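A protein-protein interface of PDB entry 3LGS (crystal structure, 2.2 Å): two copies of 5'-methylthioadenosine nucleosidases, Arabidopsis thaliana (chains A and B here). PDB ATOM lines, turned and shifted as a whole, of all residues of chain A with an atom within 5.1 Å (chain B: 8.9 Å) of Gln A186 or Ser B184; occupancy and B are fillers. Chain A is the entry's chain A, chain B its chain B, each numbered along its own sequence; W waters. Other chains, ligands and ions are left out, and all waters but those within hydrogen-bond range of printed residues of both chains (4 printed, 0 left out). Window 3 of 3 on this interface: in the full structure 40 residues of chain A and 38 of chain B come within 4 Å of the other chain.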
ATOM      1  N   ARG A 142       0.649   4.497  27.682  1.00  0.00           N
ATOM      2  CA  ARG A 142       1.063   5.769  28.264  1.00  0.00           C
ATOM      3  C   ARG A 142       0.141   6.880  27.753  1.00  0.00           C
ATOM      4  O   ARG A 142       0.131   7.183  26.552  1.00  0.00           O
ATOM      5  CB  ARG A 142       2.504   6.079  27.879  1.00  0.00           C
ATOM      6  CG  ARG A 142       3.499   4.902  28.049  1.00  0.00           C
ATOM      7  CD  ARG A 142       4.897   5.290  27.567  1.00  0.00           C
ATOM      8  NE  ARG A 142       4.898   5.752  26.179  1.00  0.00           N
ATOM      9  CZ  ARG A 142       4.952   4.954  25.111  1.00  0.00           C
ATOM     10  NH1 ARG A 142       5.004   3.644  25.257  1.00  0.00           N
ATOM     11  NH2 ARG A 142       4.941   5.467  23.882  1.00  0.00           N
ATOM     12  N   SER A 184      11.286  -2.133  25.067  1.00  0.00           N
ATOM     13  CA  SER A 184      11.888  -0.841  24.698  1.00  0.00           C
ATOM     14  C   SER A 184      12.365  -0.137  25.968  1.00  0.00           C
ATOM     15  O   SER A 184      11.975  -0.516  27.093  1.00  0.00           O
ATOM     16  CB  SER A 184      10.865   0.044  23.974  1.00  0.00           C
ATOM     17  OG  SER A 184       9.922   0.559  24.894  1.00  0.00           O
ATOM     18  N   THR A 185      13.177   0.895  25.802  1.00  0.00           N
ATOM     19  CA  THR A 185      13.670   1.657  26.952  1.00  0.00           C
ATOM     20  C   THR A 185      12.535   2.335  27.720  1.00  0.00           C
ATOM     21  O   THR A 185      12.599   2.474  28.951  1.00  0.00           O
ATOM     22  CB  THR A 185      14.700   2.700  26.536  1.00  0.00           C
ATOM     23  OG1 THR A 185      14.129   3.580  25.549  1.00  0.00           O
ATOM     24  CG2 THR A 185      15.974   1.996  25.992  1.00  0.00           C
ATOM     25  N   GLN A 186      11.491   2.728  26.995  1.00  0.00           N
ATOM     26  CA  GLN A 186      10.334   3.368  27.608  1.00  0.00           C
ATOM     27  C   GLN A 186       9.540   2.355  28.446  1.00  0.00           C
ATOM     28  O   GLN A 186       9.186   2.664  29.584  1.00  0.00           O
ATOM     29  CB  GLN A 186       9.456   4.077  26.558  1.00  0.00           C
ATOM     30  CG  GLN A 186       8.194   4.730  27.122  1.00  0.00           C
ATOM     31  CD  GLN A 186       8.490   5.938  27.998  1.00  0.00           C
ATOM     32  OE1 GLN A 186       8.763   7.034  27.501  1.00  0.00           O
ATOM     33  NE2 GLN A 186       8.438   5.740  29.308  1.00  0.00           N
ATOM     34  N   ASP A 187       9.302   1.158  27.898  1.00  0.00           N
ATOM     35  CA  ASP A 187       8.716   0.047  28.635  1.00  0.00           C
ATOM     36  C   ASP A 187       9.466  -0.222  29.948  1.00  0.00           C
ATOM     37  O   ASP A 187       8.847  -0.377  31.001  1.00  0.00           O
ATOM     38  CB  ASP A 187       8.734  -1.257  27.800  1.00  0.00           C
ATOM     39  CG  ASP A 187       7.966  -1.158  26.498  1.00  0.00           C
ATOM     40  OD1 ASP A 187       7.029  -0.322  26.383  1.00  0.00           O
ATOM     41  OD2 ASP A 187       8.292  -1.952  25.576  1.00  0.00           O
ATOM     42  N   GLU A 188      10.794  -0.297  29.871  1.00  0.00           N
ATOM     43  CA  GLU A 188      11.630  -0.650  31.024  1.00  0.00           C
ATOM     44  C   GLU A 188      11.462   0.365  32.144  1.00  0.00           C
ATOM     45  O   GLU A 188      11.265   0.001  33.314  1.00  0.00           O
ATOM     46  CB  GLU A 188      13.116  -0.728  30.628  1.00  0.00           C
ATOM     47  CG  GLU A 188      14.030  -1.075  31.808  1.00  0.00           C
ATOM     48  CD  GLU A 188      15.442  -1.482  31.410  1.00  0.00           C
ATOM     49  OE1 GLU A 188      16.012  -0.901  30.452  1.00  0.00           O
ATOM     50  OE2 GLU A 188      15.989  -2.380  32.081  1.00  0.00           O
ATOM     51  N   THR A 189      11.545   1.642  31.778  1.00  0.00           N
ATOM     52  CA  THR A 189      11.394   2.717  32.762  1.00  0.00           C
ATOM     53  C   THR A 189      10.117   2.503  33.557  1.00  0.00           C
ATOM     54  O   THR A 189      10.118   2.601  34.785  1.00  0.00           O
ATOM     55  CB  THR A 189      11.397   4.098  32.089  1.00  0.00           C
ATOM     56  OG1 THR A 189      12.657   4.287  31.450  1.00  0.00           O
ATOM     57  CG2 THR A 189      11.181   5.235  33.122  1.00  0.00           C
ATOM     58  N   LEU A 190       9.030   2.180  32.863  1.00  0.00           N
ATOM     59  CA  LEU A 190       7.759   2.023  33.547  1.00  0.00           C
ATOM     60  C   LEU A 190       7.698   0.698  34.303  1.00  0.00           C
ATOM     61  O   LEU A 190       7.088   0.620  35.363  1.00  0.00           O
ATOM     62  CB  LEU A 190       6.591   2.163  32.583  1.00  0.00           C
ATOM     63  CG  LEU A 190       6.393   3.545  31.945  1.00  0.00           C
ATOM     64  CD1 LEU A 190       5.338   3.426  30.872  1.00  0.00           C
ATOM     65  CD2 LEU A 190       5.986   4.626  32.966  1.00  0.00           C
ATOM     66  N   HIS B 139       1.918  -0.070  15.722  1.00  0.00           N
ATOM     67  CA  HIS B 139       3.321   0.253  15.973  1.00  0.00           C
ATOM     68  C   HIS B 139       3.839  -0.272  17.329  1.00  0.00           C
ATOM     69  O   HIS B 139       5.030  -0.141  17.627  1.00  0.00           O
ATOM     70  CB  HIS B 139       3.610   1.771  15.826  1.00  0.00           C
ATOM     71  CG  HIS B 139       2.617   2.658  16.518  1.00  0.00           C
ATOM     72  ND1 HIS B 139       2.735   3.022  17.849  1.00  0.00           N
ATOM     73  CD2 HIS B 139       1.489   3.254  16.064  1.00  0.00           C
ATOM     74  CE1 HIS B 139       1.721   3.804  18.177  1.00  0.00           C
ATOM     75  NE2 HIS B 139       0.947   3.953  17.115  1.00  0.00           N
ATOM     76  N   ASP B 140       2.965  -0.881  18.133  1.00  0.00           N
ATOM     77  CA  ASP B 140       3.342  -1.253  19.517  1.00  0.00           C
ATOM     78  C   ASP B 140       3.095  -2.708  19.904  1.00  0.00           C
ATOM     79  O   ASP B 140       2.911  -3.027  21.093  1.00  0.00           O
ATOM     80  CB  ASP B 140       2.686  -0.295  20.534  1.00  0.00           C
ATOM     81  CG  ASP B 140       1.225  -0.654  20.869  1.00  0.00           C
ATOM     82  OD1 ASP B 140       0.542  -1.375  20.078  1.00  0.00           O
ATOM     83  OD2 ASP B 140       0.764  -0.182  21.936  1.00  0.00           O
ATOM     84  N   ARG B 142       5.394  -5.482  19.223  1.00  0.00           N
ATOM     85  CA  ARG B 142       6.712  -5.858  18.683  1.00  0.00           C
ATOM     86  C   ARG B 142       7.062  -7.257  19.153  1.00  0.00           C
ATOM     87  O   ARG B 142       7.316  -7.490  20.345  1.00  0.00           O
ATOM     88  CB  ARG B 142       7.810  -4.887  19.129  1.00  0.00           C
ATOM     89  CG  ARG B 142       7.720  -3.466  18.564  1.00  0.00           C
ATOM     90  CD  ARG B 142       8.714  -2.529  19.241  1.00  0.00           C
ATOM     91  NE  ARG B 142       8.908  -2.927  20.628  1.00  0.00           N
ATOM     92  CZ  ARG B 142       8.382  -2.310  21.676  1.00  0.00           C
ATOM     93  NH1 ARG B 142       7.663  -1.218  21.523  1.00  0.00           N
ATOM     94  NH2 ARG B 142       8.589  -2.787  22.886  1.00  0.00           N
ATOM     95  N   SER B 180      -0.611   4.134  23.400  1.00  0.00           N
ATOM     96  CA  SER B 180      -0.050   5.362  23.998  1.00  0.00           C
ATOM     97  C   SER B 180      -0.361   6.627  23.172  1.00  0.00           C
ATOM     98  O   SER B 180      -0.352   6.613  21.935  1.00  0.00           O
ATOM     99  CB  SER B 180       1.466   5.230  24.211  1.00  0.00           C
ATOM    100  OG  SER B 180       1.776   4.127  25.062  1.00  0.00           O
ATOM    101  N   LEU B 181      -0.653   7.715  23.872  1.00  0.00           N
ATOM    102  CA  LEU B 181      -0.946   8.988  23.229  1.00  0.00           C
ATOM    103  C   LEU B 181       0.352   9.671  22.776  1.00  0.00           C
ATOM    104  O   LEU B 181       0.397  10.260  21.681  1.00  0.00           O
ATOM    105  CB  LEU B 181      -1.756   9.888  24.169  1.00  0.00           C
ATOM    106  CG  LEU B 181      -2.177  11.276  23.667  1.00  0.00           C
ATOM    107  CD1 LEU B 181      -3.033  11.195  22.392  1.00  0.00           C
ATOM    108  CD2 LEU B 181      -2.945  12.001  24.750  1.00  0.00           C
ATOM    109  N   ASP B 182       1.395   9.583  23.614  1.00  0.00           N
ATOM    110  CA  ASP B 182       2.722  10.071  23.252  1.00  0.00           C
ATOM    111  C   ASP B 182       3.429   9.060  22.333  1.00  0.00           C
ATOM    112  O   ASP B 182       2.831   8.058  21.904  1.00  0.00           O
ATOM    113  CB  ASP B 182       3.563  10.359  24.512  1.00  0.00           C
ATOM    114  CG  ASP B 182       3.911   9.083  25.316  1.00  0.00           C
ATOM    115  OD1 ASP B 182       3.418   7.990  24.993  1.00  0.00           O
ATOM    116  OD2 ASP B 182       4.703   9.171  26.283  1.00  0.00           O
ATOM    117  N   MET B 183       4.703   9.313  22.047  1.00  0.00           N
ATOM    118  CA  MET B 183       5.439   8.502  21.095  1.00  0.00           C
ATOM    119  C   MET B 183       6.868   8.274  21.583  1.00  0.00           C
ATOM    120  O   MET B 183       7.654   9.207  21.673  1.00  0.00           O
ATOM    121  CB  MET B 183       5.429   9.200  19.729  1.00  0.00           C
ATOM    122  CG  MET B 183       6.023   8.391  18.591  1.00  0.00           C
ATOM    123  SD  MET B 183       5.932   9.246  16.985  1.00  0.00           S
ATOM    124  CE  MET B 183       7.042  10.639  17.308  1.00  0.00           C
ATOM    125  N   SER B 184       7.210   7.035  21.906  1.00  0.00           N
ATOM    126  CA  SER B 184       8.586   6.746  22.337  1.00  0.00           C
ATOM    127  C   SER B 184       9.492   6.698  21.094  1.00  0.00           C
ATOM    128  O   SER B 184       8.997   6.683  19.968  1.00  0.00           O
ATOM    129  CB  SER B 184       8.645   5.436  23.138  1.00  0.00           C
ATOM    130  OG  SER B 184       8.600   4.296  22.275  1.00  0.00           O
ATOM    131  N   THR B 185      10.806   6.706  21.298  1.00  0.00           N
ATOM    132  CA  THR B 185      11.751   6.570  20.203  1.00  0.00           C
ATOM    133  C   THR B 185      11.439   5.322  19.361  1.00  0.00           C
ATOM    134  O   THR B 185      11.283   5.408  18.131  1.00  0.00           O
ATOM    135  CB  THR B 185      13.204   6.519  20.713  1.00  0.00           C
ATOM    136  OG1 THR B 185      13.475   7.668  21.524  1.00  0.00           O
ATOM    137  CG2 THR B 185      14.195   6.479  19.521  1.00  0.00           C
ATOM    138  N   GLN B 186      11.311   4.177  20.018  1.00  0.00           N
ATOM    139  CA  GLN B 186      10.993   2.938  19.294  1.00  0.00           C
ATOM    140  C   GLN B 186       9.699   3.048  18.469  1.00  0.00           C
ATOM    141  O   GLN B 186       9.652   2.561  17.326  1.00  0.00           O
ATOM    142  CB  GLN B 186      10.962   1.732  20.237  1.00  0.00           C
ATOM    143  CG  GLN B 186      10.534   0.398  19.581  1.00  0.00           C
ATOM    144  CD  GLN B 186      11.575  -0.194  18.632  1.00  0.00           C
ATOM    145  OE1 GLN B 186      12.546  -0.811  19.064  1.00  0.00           O
ATOM    146  NE2 GLN B 186      11.355  -0.023  17.330  1.00  0.00           N
ATOM    147  N   ASP B 187       8.670   3.680  19.047  1.00  0.00           N
ATOM    148  CA  ASP B 187       7.386   3.857  18.381  1.00  0.00           C
ATOM    149  C   ASP B 187       7.595   4.607  17.079  1.00  0.00           C
ATOM    150  O   ASP B 187       7.057   4.224  16.041  1.00  0.00           O
ATOM    151  CB  ASP B 187       6.401   4.679  19.223  1.00  0.00           C
ATOM    152  CG  ASP B 187       5.905   3.964  20.455  1.00  0.00           C
ATOM    153  OD1 ASP B 187       5.886   2.704  20.494  1.00  0.00           O
ATOM    154  OD2 ASP B 187       5.496   4.701  21.388  1.00  0.00           O
ATOM    155  N   GLU B 188       8.373   5.682  17.160  1.00  0.00           N
ATOM    156  CA  GLU B 188       8.593   6.596  16.047  1.00  0.00           C
ATOM    157  C   GLU B 188       9.354   5.932  14.900  1.00  0.00           C
ATOM    158  O   GLU B 188       9.030   6.129  13.742  1.00  0.00           O
ATOM    159  CB  GLU B 188       9.352   7.845  16.532  1.00  0.00           C
ATOM    160  CG  GLU B 188       9.723   8.815  15.400  1.00  0.00           C
ATOM    161  CD  GLU B 188      10.658   9.934  15.835  1.00  0.00           C
ATOM    162  OE1 GLU B 188      11.704   9.669  16.482  1.00  0.00           O
ATOM    163  OE2 GLU B 188      10.350  11.085  15.501  1.00  0.00           O
ATOM    164  N   THR B 189      10.380   5.163  15.232  1.00  0.00           N
ATOM    165  CA  THR B 189      11.123   4.408  14.243  1.00  0.00           C
ATOM    166  C   THR B 189      10.150   3.492  13.457  1.00  0.00           C
ATOM    167  O   THR B 189      10.159   3.495  12.223  1.00  0.00           O
ATOM    168  CB  THR B 189      12.266   3.597  14.928  1.00  0.00           C
ATOM    169  OG1 THR B 189      13.161   4.499  15.605  1.00  0.00           O
ATOM    170  CG2 THR B 189      13.054   2.755  13.908  1.00  0.00           C
ATOM    171  N   LEU B 190       9.297   2.743  14.171  1.00  0.00           N
ATOM    172  CA  LEU B 190       8.323   1.867  13.508  1.00  0.00           C
ATOM    173  C   LEU B 190       7.251   2.623  12.730  1.00  0.00           C
ATOM    174  O   LEU B 190       6.825   2.160  11.690  1.00  0.00           O
ATOM    175  CB  LEU B 190       7.674   0.888  14.486  1.00  0.00           C
ATOM    176  CG  LEU B 190       8.597  -0.174  15.090  1.00  0.00           C
ATOM    177  CD1 LEU B 190       7.895  -0.881  16.204  1.00  0.00           C
ATOM    178  CD2 LEU B 190       9.091  -1.184  14.040  1.00  0.00           C
ATOM    179  N   ILE B 191       6.807   3.766  13.239  1.00  0.00           N
ATOM    180  CA  ILE B 191       5.820   4.584  12.524  1.00  0.00           C
ATOM    181  C   ILE B 191       6.404   5.209  11.229  1.00  0.00           C
ATOM    182  O   ILE B 191       5.726   5.293  10.207  1.00  0.00           O
ATOM    183  CB  ILE B 191       5.219   5.654  13.441  1.00  0.00           C
ATOM    184  CG1 ILE B 191       4.418   4.971  14.542  1.00  0.00           C
ATOM    185  CG2 ILE B 191       4.324   6.607  12.653  1.00  0.00           C
ATOM    186  CD1 ILE B 191       4.123   5.804  15.716  1.00  0.00           C
ATOM    187  N   ILE B 192       7.659   5.631  11.276  1.00  0.00           N
ATOM    188  CA  ILE B 192       8.316   6.182  10.093  1.00  0.00           C
ATOM    189  C   ILE B 192       8.530   5.059   9.089  1.00  0.00           C
ATOM    190  O   ILE B 192       8.224   5.218   7.911  1.00  0.00           O
ATOM    191  CB  ILE B 192       9.633   6.910  10.446  1.00  0.00           C
ATOM    192  CG1 ILE B 192       9.318   8.230  11.151  1.00  0.00           C
ATOM    193  CG2 ILE B 192      10.513   7.148   9.185  1.00  0.00           C
ATOM    194  CD1 ILE B 192      10.510   8.877  11.828  1.00  0.00           C
ATOM    195  N   LYS B 199      -1.694   8.516  13.285  1.00  0.00           N
ATOM    196  CA  LYS B 199      -1.421   7.749  14.507  1.00  0.00           C
ATOM    197  C   LYS B 199      -2.633   7.805  15.432  1.00  0.00           C
ATOM    198  O   LYS B 199      -3.043   8.900  15.822  1.00  0.00           O
ATOM    199  CB  LYS B 199      -0.205   8.350  15.220  1.00  0.00           C
ATOM    200  CG  LYS B 199       0.270   7.624  16.501  1.00  0.00           C
ATOM    201  CD  LYS B 199       1.582   8.216  17.017  1.00  0.00           C
ATOM    202  CE  LYS B 199       1.947   7.665  18.394  1.00  0.00           C
ATOM    203  NZ  LYS B 199       0.897   7.922  19.454  1.00  0.00           N
ATOM    204  N   VAL B 227       2.284  15.312  14.927  1.00  0.00           N
ATOM    205  CA  VAL B 227       3.276  14.488  15.611  1.00  0.00           C
ATOM    206  C   VAL B 227       4.715  14.914  15.270  1.00  0.00           C
ATOM    207  O   VAL B 227       5.634  14.721  16.082  1.00  0.00           O
ATOM    208  CB  VAL B 227       3.031  12.971  15.331  1.00  0.00           C
ATOM    209  CG1 VAL B 227       4.111  12.122  15.976  1.00  0.00           C
ATOM    210  CG2 VAL B 227       1.653  12.548  15.834  1.00  0.00           C
HETATM  211  O   HOH W   1       6.029  -0.634  23.814  1.00  0.00           O
HETATM  212  O   HOH W   2       8.213   2.162  23.592  1.00  0.00           O
HETATM  213  O   HOH W   3       4.959   1.734  23.059  1.00  0.00           O
HETATM  214  O   HOH W   4       7.520   8.012  25.397  1.00  0.00           O
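Of chain B, only Ser B184 comes within 4 Å of Gln A186.
Of chain A, only Arg A142 and Gln A186 come within 4 Å of Ser B184.
Thr A185 touches none of the printed residues of chain B.
Printed residues of chain B within 4 Å of Ser A184: Arg B142 (3.5 Å).
Of the printed residues of chain A, Asp B182 touches Arg A142.
Of the printed residues of chain B, Arg A142 touches Ser B180, Leu B181, Asp B182, Ser B184 and Asp B187.
Glu B188 touches none of the printed residues of chain A.
The nearest residue of chain B that does not touch Gln A186 is Asp B182 (4.7 Å).
Arg A142 touches Ser B184, and with the chains exchanged Ser A184 touches Arg B142.
Arg A142 touches Asp B187, and with the chains exchanged Asp A187 touches Arg B142.
Gln A186 touches Ser B184, but with the chains exchanged Ser A184 does not touch Gln B186 (4.1 Å).
Of the 8 pairs that touch across the chains among the printed residues, 4 have their exchanged pair printed and touching as well.
Water W2 bridges the side-chain hydroxyl (OG) of Ser B184 (2.5 Å) and the side-chain hydroxyl (OG) of Ser A184 (2.7 Å).
Water W4 bridges the side-chain amide oxygen (OE1) of Gln A186 (2.6 Å) and the side-chain carboxylate (OD2) of Asp B182 (3.2 Å).
Water W1 lies within hydrogen-bond range of OD1 of Asp A187 (2.8 Å) and NH1 of Arg B142 (2.9 Å).
Water W3 lies within hydrogen-bond range of the side-chain carboxylate (OD1) of Asp B187 (2.9 Å) and the guanidinium group (NH1) of Arg A142 (2.9 Å).
The side-chain hydroxyl (OG) of Ser B180 lies within hydrogen-bond range of the backbone NH (N) of Arg A142.
NH2 of Arg B142 is in salt-bridge range of OD2 of Asp A187 (2.8 Å).
The side-chain carboxylate (OD2) of Asp B187 lies within salt-bridge range of the guanidinium group (NH2) of Arg A142, 2.7 Å away.
OD1 of Asp B182 is in salt-bridge range of NE of Arg A142 (2.9 Å).
The backbone NH (N) of Ser B184 sits close to the guanidinium group (NH2) of Arg A142 (3.4 Å).
O of Arg A142 sits at hydrogen-bond distance from N of Leu B181.
Of the 18 printed residues of chain B, 6 touch a printed residue of chain A.
Along chain B the printed residues that touch a printed residue of chain A span positions 142 to 187.
Among the printed residues, Asp or Glu carboxylates within 4 Å of a Lys or Arg side-chain nitrogen of the other chain: Arg A142 with Asp B182, Arg A142 with Asp B187 and Asp A187 with Arg B142.
Among the printed residues, merely in contact across the chains: Ser A184 with Arg B142 (3.5 Å) and Gln A186 with Ser B184 (3.8 Å).
The side-chain carboxylate (OD2) of Asp B187 lies within hydrogen-bond range of the backbone NH (N) of Ser B184, 2.9 Å away.
The backbone carbonyl oxygen (O) of Asp B182 sits at hydrogen-bond distance from the side-chain amino group (NZ) of Lys B199 (3.1 Å).
The backbone NH (N) of Ser A184 lies within hydrogen-bond range of the side-chain carboxylate (OD2) of Asp A187, at 3.0 Å.
NZ of Lys B199 is in hydrogen-bond range of O of Leu B181, 3.3 Å away.
The backbone NH (N) of Gln A186 lies close to the side-chain hydroxyl (OG) of Ser A184 (3.4 Å).
The side-chain amino group of Lys B199 sits at hydrogen-bond distance from the backbone carbonyl oxygen of Ser B180 (3.1 Å).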
